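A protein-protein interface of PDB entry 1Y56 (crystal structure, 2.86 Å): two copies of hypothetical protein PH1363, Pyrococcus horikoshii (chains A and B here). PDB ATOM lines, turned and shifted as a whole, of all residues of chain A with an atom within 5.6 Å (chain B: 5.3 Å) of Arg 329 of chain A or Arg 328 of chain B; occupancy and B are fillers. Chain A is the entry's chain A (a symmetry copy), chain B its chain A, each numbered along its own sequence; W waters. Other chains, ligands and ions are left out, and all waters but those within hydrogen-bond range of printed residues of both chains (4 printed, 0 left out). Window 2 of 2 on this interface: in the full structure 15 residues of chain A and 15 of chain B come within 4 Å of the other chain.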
ATOM      1  N   PHE A 327      16.174  15.908 -22.016  1.00  0.00           N
ATOM      2  CA  PHE A 327      16.806  17.180 -21.658  1.00  0.00           C
ATOM      3  C   PHE A 327      15.980  18.345 -22.166  1.00  0.00           C
ATOM      4  O   PHE A 327      15.741  18.458 -23.369  1.00  0.00           O
ATOM      5  CB  PHE A 327      18.236  17.278 -22.183  1.00  0.00           C
ATOM      6  CG  PHE A 327      18.967  18.505 -21.713  1.00  0.00           C
ATOM      7  CD1 PHE A 327      19.506  18.564 -20.429  1.00  0.00           C
ATOM      8  CD2 PHE A 327      19.121  19.607 -22.550  1.00  0.00           C
ATOM      9  CE1 PHE A 327      20.184  19.706 -19.983  1.00  0.00           C
ATOM     10  CE2 PHE A 327      19.795  20.749 -22.113  1.00  0.00           C
ATOM     11  CZ  PHE A 327      20.327  20.795 -20.825  1.00  0.00           C
ATOM     12  N   ARG A 328      15.535  19.195 -21.242  1.00  0.00           N
ATOM     13  CA  ARG A 328      14.763  20.403 -21.559  1.00  0.00           C
ATOM     14  C   ARG A 328      14.871  21.431 -20.445  1.00  0.00           C
ATOM     15  O   ARG A 328      14.878  21.076 -19.265  1.00  0.00           O
ATOM     16  CB  ARG A 328      13.283  20.091 -21.829  1.00  0.00           C
ATOM     17  CG  ARG A 328      12.932  20.000 -23.318  1.00  0.00           C
ATOM     18  CD  ARG A 328      11.417  19.921 -23.579  1.00  0.00           C
ATOM     19  NE  ARG A 328      10.688  21.121 -23.128  1.00  0.00           N
ATOM     20  CZ  ARG A 328       9.352  21.238 -23.053  1.00  0.00           C
ATOM     21  NH1 ARG A 328       8.822  22.380 -22.613  1.00  0.00           N
ATOM     22  NH2 ARG A 328       8.543  20.230 -23.402  1.00  0.00           N
ATOM     23  N   ARG A 329      14.937  22.702 -20.841  1.00  0.00           N
ATOM     24  CA  ARG A 329      14.979  23.833 -19.925  1.00  0.00           C
ATOM     25  C   ARG A 329      16.202  23.822 -19.045  1.00  0.00           C
ATOM     26  O   ARG A 329      16.164  24.319 -17.930  1.00  0.00           O
ATOM     27  CB  ARG A 329      13.718  23.913 -19.067  1.00  0.00           C
ATOM     28  CG  ARG A 329      12.511  24.266 -19.854  1.00  0.00           C
ATOM     29  CD  ARG A 329      11.219  24.161 -19.057  1.00  0.00           C
ATOM     30  NE  ARG A 329      10.075  24.414 -19.939  1.00  0.00           N
ATOM     31  CZ  ARG A 329       9.708  25.627 -20.382  1.00  0.00           C
ATOM     32  NH1 ARG A 329      10.368  26.736 -20.018  1.00  0.00           N
ATOM     33  NH2 ARG A 329       8.663  25.735 -21.197  1.00  0.00           N
ATOM     34  N   GLY A 330      17.292  23.275 -19.558  1.00  0.00           N
ATOM     35  CA  GLY A 330      18.563  23.292 -18.855  1.00  0.00           C
ATOM     36  C   GLY A 330      18.766  22.136 -17.891  1.00  0.00           C
ATOM     37  O   GLY A 330      19.725  22.142 -17.119  1.00  0.00           O
ATOM     38  N   TYR A 331      17.885  21.137 -17.931  1.00  0.00           N
ATOM     39  CA  TYR A 331      17.988  19.992 -17.025  1.00  0.00           C
ATOM     40  C   TYR A 331      17.295  18.732 -17.492  1.00  0.00           C
ATOM     41  O   TYR A 331      16.383  18.784 -18.298  1.00  0.00           O
ATOM     42  CB  TYR A 331      17.500  20.360 -15.628  1.00  0.00           C
ATOM     43  CG  TYR A 331      16.111  20.924 -15.547  1.00  0.00           C
ATOM     44  CD1 TYR A 331      15.005  20.084 -15.381  1.00  0.00           C
ATOM     45  CD2 TYR A 331      15.901  22.296 -15.579  1.00  0.00           C
ATOM     46  CE1 TYR A 331      13.714  20.599 -15.270  1.00  0.00           C
ATOM     47  CE2 TYR A 331      14.614  22.830 -15.473  1.00  0.00           C
ATOM     48  CZ  TYR A 331      13.524  21.977 -15.318  1.00  0.00           C
ATOM     49  OH  TYR A 331      12.254  22.506 -15.212  1.00  0.00           O
ATOM     50  N   GLU A 393       4.471  28.149 -15.563  1.00  0.00           N
ATOM     51  CA  GLU A 393       5.439  27.725 -16.550  1.00  0.00           C
ATOM     52  C   GLU A 393       6.636  27.190 -15.785  1.00  0.00           C
ATOM     53  O   GLU A 393       7.137  27.861 -14.892  1.00  0.00           O
ATOM     54  CB  GLU A 393       5.853  28.883 -17.456  1.00  0.00           C
ATOM     55  CG  GLU A 393       6.921  28.507 -18.481  1.00  0.00           C
ATOM     56  CD  GLU A 393       7.456  29.693 -19.265  1.00  0.00           C
ATOM     57  OE1 GLU A 393       8.309  29.466 -20.149  1.00  0.00           O
ATOM     58  OE2 GLU A 393       7.033  30.843 -19.006  1.00  0.00           O
ATOM     59  N   PRO A 394       7.077  25.969 -16.113  1.00  0.00           N
ATOM     60  CA  PRO A 394       8.274  25.411 -15.491  1.00  0.00           C
ATOM     61  C   PRO A 394       9.521  26.246 -15.782  1.00  0.00           C
ATOM     62  O   PRO A 394       9.721  26.687 -16.918  1.00  0.00           O
ATOM     63  CB  PRO A 394       8.384  24.018 -16.124  1.00  0.00           C
ATOM     64  CG  PRO A 394       7.554  24.074 -17.360  1.00  0.00           C
ATOM     65  CD  PRO A 394       6.461  25.036 -17.069  1.00  0.00           C
ATOM     66  N   GLU A 395      10.341  26.454 -14.749  1.00  0.00           N
ATOM     67  CA  GLU A 395      11.554  27.287 -14.822  1.00  0.00           C
ATOM     68  C   GLU A 395      12.683  26.675 -15.628  1.00  0.00           C
ATOM     69  O   GLU A 395      12.823  25.456 -15.684  1.00  0.00           O
ATOM     70  CB  GLU A 395      12.086  27.577 -13.423  1.00  0.00           C
ATOM     71  CG  GLU A 395      11.355  28.686 -12.685  1.00  0.00           C
ATOM     72  CD  GLU A 395      11.529  28.592 -11.165  1.00  0.00           C
ATOM     73  OE1 GLU A 395      10.483  28.598 -10.460  1.00  0.00           O
ATOM     74  OE2 GLU A 395      12.698  28.500 -10.687  1.00  0.00           O
ATOM     75  N   SER A 396      13.500  27.538 -16.231  1.00  0.00           N
ATOM     76  CA  SER A 396      14.718  27.108 -16.918  1.00  0.00           C
ATOM     77  C   SER A 396      15.943  27.261 -16.024  1.00  0.00           C
ATOM     78  O   SER A 396      15.904  27.916 -14.995  1.00  0.00           O
ATOM     79  CB  SER A 396      14.935  27.911 -18.197  1.00  0.00           C
ATOM     80  OG  SER A 396      13.714  28.171 -18.861  1.00  0.00           O
ATOM     81  N   LEU A 397      17.032  26.633 -16.427  1.00  0.00           N
ATOM     82  CA  LEU A 397      18.309  26.853 -15.800  1.00  0.00           C
ATOM     83  C   LEU A 397      19.308  27.128 -16.891  1.00  0.00           C
ATOM     84  O   LEU A 397      19.347  26.410 -17.891  1.00  0.00           O
ATOM     85  CB  LEU A 397      18.750  25.627 -15.007  1.00  0.00           C
ATOM     86  CG  LEU A 397      18.209  25.471 -13.592  1.00  0.00           C
ATOM     87  CD1 LEU A 397      18.857  24.273 -12.926  1.00  0.00           C
ATOM     88  CD2 LEU A 397      18.456  26.734 -12.781  1.00  0.00           C
ATOM     89  N   ARG B 326       2.127  36.182 -26.287  1.00  0.00           N
ATOM     90  CA  ARG B 326       2.190  35.162 -25.258  1.00  0.00           C
ATOM     91  C   ARG B 326       3.502  35.404 -24.502  1.00  0.00           C
ATOM     92  O   ARG B 326       4.527  35.718 -25.123  1.00  0.00           O
ATOM     93  CB  ARG B 326       2.258  33.811 -25.953  1.00  0.00           C
ATOM     94  CG  ARG B 326       1.535  32.666 -25.278  1.00  0.00           C
ATOM     95  CD  ARG B 326       2.178  31.293 -25.604  1.00  0.00           C
ATOM     96  NE  ARG B 326       2.782  31.190 -26.946  1.00  0.00           N
ATOM     97  CZ  ARG B 326       4.076  31.405 -27.230  1.00  0.00           C
ATOM     98  NH1 ARG B 326       4.941  31.759 -26.282  1.00  0.00           N
ATOM     99  NH2 ARG B 326       4.512  31.285 -28.479  1.00  0.00           N
ATOM    100  N   PHE B 327       3.494  35.273 -23.178  1.00  0.00           N
ATOM    101  CA  PHE B 327       4.759  35.308 -22.440  1.00  0.00           C
ATOM    102  C   PHE B 327       5.235  33.902 -22.134  1.00  0.00           C
ATOM    103  O   PHE B 327       4.528  33.137 -21.478  1.00  0.00           O
ATOM    104  CB  PHE B 327       4.649  36.121 -21.152  1.00  0.00           C
ATOM    105  CG  PHE B 327       5.961  36.303 -20.441  1.00  0.00           C
ATOM    106  CD1 PHE B 327       6.883  37.251 -20.882  1.00  0.00           C
ATOM    107  CD2 PHE B 327       6.282  35.528 -19.330  1.00  0.00           C
ATOM    108  CE1 PHE B 327       8.110  37.422 -20.227  1.00  0.00           C
ATOM    109  CE2 PHE B 327       7.504  35.692 -18.673  1.00  0.00           C
ATOM    110  CZ  PHE B 327       8.417  36.643 -19.125  1.00  0.00           C
ATOM    111  N   ARG B 328       6.427  33.567 -22.628  1.00  0.00           N
ATOM    112  CA  ARG B 328       7.063  32.265 -22.387  1.00  0.00           C
ATOM    113  C   ARG B 328       8.569  32.351 -22.569  1.00  0.00           C
ATOM    114  O   ARG B 328       9.053  33.043 -23.466  1.00  0.00           O
ATOM    115  CB  ARG B 328       6.497  31.167 -23.300  1.00  0.00           C
ATOM    116  CG  ARG B 328       5.439  30.287 -22.625  1.00  0.00           C
ATOM    117  CD  ARG B 328       5.053  29.054 -23.463  1.00  0.00           C
ATOM    118  NE  ARG B 328       6.178  28.128 -23.685  1.00  0.00           N
ATOM    119  CZ  ARG B 328       6.175  27.087 -24.533  1.00  0.00           C
ATOM    120  NH1 ARG B 328       7.270  26.335 -24.647  1.00  0.00           N
ATOM    121  NH2 ARG B 328       5.099  26.795 -25.274  1.00  0.00           N
ATOM    122  N   ARG B 329       9.293  31.623 -21.717  1.00  0.00           N
ATOM    123  CA  ARG B 329      10.744  31.522 -21.771  1.00  0.00           C
ATOM    124  C   ARG B 329      11.428  32.847 -21.550  1.00  0.00           C
ATOM    125  O   ARG B 329      12.513  33.074 -22.058  1.00  0.00           O
ATOM    126  CB  ARG B 329      11.220  30.901 -23.082  1.00  0.00           C
ATOM    127  CG  ARG B 329      10.859  29.467 -23.201  1.00  0.00           C
ATOM    128  CD  ARG B 329      11.151  28.882 -24.576  1.00  0.00           C
ATOM    129  NE  ARG B 329      10.661  27.503 -24.638  1.00  0.00           N
ATOM    130  CZ  ARG B 329      11.263  26.452 -24.059  1.00  0.00           C
ATOM    131  NH1 ARG B 329      12.412  26.590 -23.378  1.00  0.00           N
ATOM    132  NH2 ARG B 329      10.716  25.246 -24.164  1.00  0.00           N
ATOM    133  N   GLY B 330      10.797  33.712 -20.770  1.00  0.00           N
ATOM    134  CA  GLY B 330      11.393  34.982 -20.395  1.00  0.00           C
ATOM    135  C   GLY B 330      11.149  36.109 -21.383  1.00  0.00           C
ATOM    136  O   GLY B 330      11.748  37.178 -21.255  1.00  0.00           O
ATOM    137  N   TYR B 331      10.269  35.894 -22.361  1.00  0.00           N
ATOM    138  CA  TYR B 331       9.986  36.915 -23.370  1.00  0.00           C
ATOM    139  C   TYR B 331       8.655  36.779 -24.073  1.00  0.00           C
ATOM    140  O   TYR B 331       8.083  35.705 -24.124  1.00  0.00           O
ATOM    141  CB  TYR B 331      11.108  36.984 -24.400  1.00  0.00           C
ATOM    142  CG  TYR B 331      11.442  35.693 -25.091  1.00  0.00           C
ATOM    143  CD1 TYR B 331      10.791  35.322 -26.273  1.00  0.00           C
ATOM    144  CD2 TYR B 331      12.445  34.867 -24.601  1.00  0.00           C
ATOM    145  CE1 TYR B 331      11.118  34.142 -26.940  1.00  0.00           C
ATOM    146  CE2 TYR B 331      12.784  33.681 -25.254  1.00  0.00           C
ATOM    147  CZ  TYR B 331      12.118  33.323 -26.424  1.00  0.00           C
ATOM    148  OH  TYR B 331      12.455  32.150 -27.069  1.00  0.00           O
ATOM    149  N   TYR B 332       8.182  37.880 -24.639  1.00  0.00           N
ATOM    150  CA  TYR B 332       6.929  37.890 -25.375  1.00  0.00           C
ATOM    151  C   TYR B 332       7.063  37.345 -26.788  1.00  0.00           C
ATOM    152  O   TYR B 332       7.957  37.720 -27.542  1.00  0.00           O
ATOM    153  CB  TYR B 332       6.353  39.295 -25.411  1.00  0.00           C
ATOM    154  CG  TYR B 332       5.806  39.752 -24.080  1.00  0.00           C
ATOM    155  CD1 TYR B 332       6.577  40.534 -23.223  1.00  0.00           C
ATOM    156  CD2 TYR B 332       4.512  39.403 -23.679  1.00  0.00           C
ATOM    157  CE1 TYR B 332       6.085  40.959 -21.999  1.00  0.00           C
ATOM    158  CE2 TYR B 332       3.997  39.825 -22.454  1.00  0.00           C
ATOM    159  CZ  TYR B 332       4.789  40.604 -21.615  1.00  0.00           C
ATOM    160  OH  TYR B 332       4.289  41.035 -20.392  1.00  0.00           O
ATOM    161  N   GLU B 393      15.711  23.386 -29.333  1.00  0.00           N
ATOM    162  CA  GLU B 393      14.861  23.891 -28.279  1.00  0.00           C
ATOM    163  C   GLU B 393      15.067  25.394 -28.233  1.00  0.00           C
ATOM    164  O   GLU B 393      16.202  25.850 -28.181  1.00  0.00           O
ATOM    165  CB  GLU B 393      15.208  23.257 -26.934  1.00  0.00           C
ATOM    166  CG  GLU B 393      14.379  23.799 -25.770  1.00  0.00           C
ATOM    167  CD  GLU B 393      14.838  23.298 -24.412  1.00  0.00           C
ATOM    168  OE1 GLU B 393      14.191  23.667 -23.409  1.00  0.00           O
ATOM    169  OE2 GLU B 393      15.836  22.544 -24.339  1.00  0.00           O
ATOM    170  N   SER B 396      15.771  30.264 -23.414  1.00  0.00           N
ATOM    171  CA  SER B 396      15.133  31.093 -22.393  1.00  0.00           C
ATOM    172  C   SER B 396      15.950  32.348 -22.106  1.00  0.00           C
ATOM    173  O   SER B 396      17.102  32.461 -22.493  1.00  0.00           O
ATOM    174  CB  SER B 396      14.950  30.314 -21.093  1.00  0.00           C
ATOM    175  OG  SER B 396      14.596  28.968 -21.339  1.00  0.00           O
HETATM  176  O   HOH W   1       4.624  32.183 -18.178  1.00  0.00           O
HETATM  177  O   HOH W   2       8.877  32.766 -19.118  1.00  0.00           O
HETATM  178  O   HOH W   3      17.132  20.437 -25.810  1.00  0.00           O
HETATM  179  O   HOH W   4      17.424  22.988 -22.243  1.00  0.00           O
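Of the 10 printed residues of chain A, 4 touch a printed residue of chain B. Printed residues of chain A that touch a printed residue of chain B: Arg 328, Arg 329, Glu 393 and Ser 396. Along chain A the printed residues that touch a printed residue of chain B span positions 328 to 396. Among the printed residues, 8 pairs touch across the chains.
Water W4 lies within hydrogen-bond range of OE2 of Glu 393 of chain B (2.7 Å), N of Gly 330 of chain A (2.7 Å) and N of Arg 329 of chain A (2.9 Å). Water W2 lies within hydrogen-bond range of OE2 of Glu 393 of chain A (2.7 Å), N of Gly 330 of chain B (2.7 Å) and N of Arg 329 of chain B (2.9 Å). Water W3 lies within hydrogen-bond range of OE2 of Glu 393 of chain B and O of Phe 327 of chain A. Water W1 lies within hydrogen-bond range of the side-chain carboxylate (OE2) of Glu 393 of chain A (2.9 Å) and the backbone carbonyl oxygen (O) of Phe 327 of chain B (3.4 Å).
Among the printed residues, pairs that only touch across the chains: Arg 328 of chain A with Arg 329 of chain B, Arg 328 of chain A with Glu 393 of chain B, Arg 329 of chain A with Arg 328 of chain B, Arg 329 of chain A with Arg 329 of chain B and Glu 393 of chain A with Arg 328 of chain B.
The side-chain carboxylate (OE1) of Glu 393 of chain B lies within salt-bridge range of the guanidinium group (NH1) of Arg 329 of chain B (3.4 Å). O of Pro 394 of chain A sits at hydrogen-bond distance from NH1 of Arg 329 of chain A (3.2 Å). The guanidinium group (NH1) of Arg 329 of chain A lies within salt-bridge range of the side-chain carboxylate (OE1) of Glu 393 of chain A, at 3.4 Å. The backbone carbonyl oxygen (O) of Arg 329 of chain A is in hydrogen-bond range of the backbone NH (N) of Leu 397 of chain A.
Arg 328 of chain A touches Arg 329 of chain B, and with the chains exchanged Arg 329 of chain A touches Arg 328 of chain B. Arg 329 of chain B touches its own counterpart, Arg 329 of chain A. Arg 329 of chain A touches Glu 393 of chain B, and with the chains exchanged Glu 393 of chain A touches Arg 329 of chain B. Ser 396 of chain A touches its own counterpart, Ser 396 of chain B. Positions printed for both chains: 327, 328, 329, 330, 331, 393 and 396. Of the 8 pairs that touch across the chains among the printed residues, 8 have their exchanged pair printed and touching as well.
Of the printed residues of chain B, Arg 328 of chain A touches Arg 329 and Glu 393. Arg 329 of chain A touches three residues of chain B. Printed residues of chain B within 4 Å of Ser 396 of chain A: Ser 396 (2.7 Å). Leu 397 of chain A touches none of the printed residues of chain B. Arg 326 of chain B touches none of the printed residues of chain A. Of the printed residues of chain A, Glu 393 of chain B touches Arg 328 and Arg 329.
OG of Ser 396 of chain A lies within hydrogen-bond range of OG of Ser 396 of chain B (2.7 Å). The side-chain carboxylate (OE1) of Glu 393 of chain B is in hydrogen-bond range of the backbone NH (N) of Arg 329 of chain A (2.8 Å). The backbone NH (N) of Arg 329 of chain B is in hydrogen-bond range of the side-chain carboxylate (OE1) of Glu 393 of chain A.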
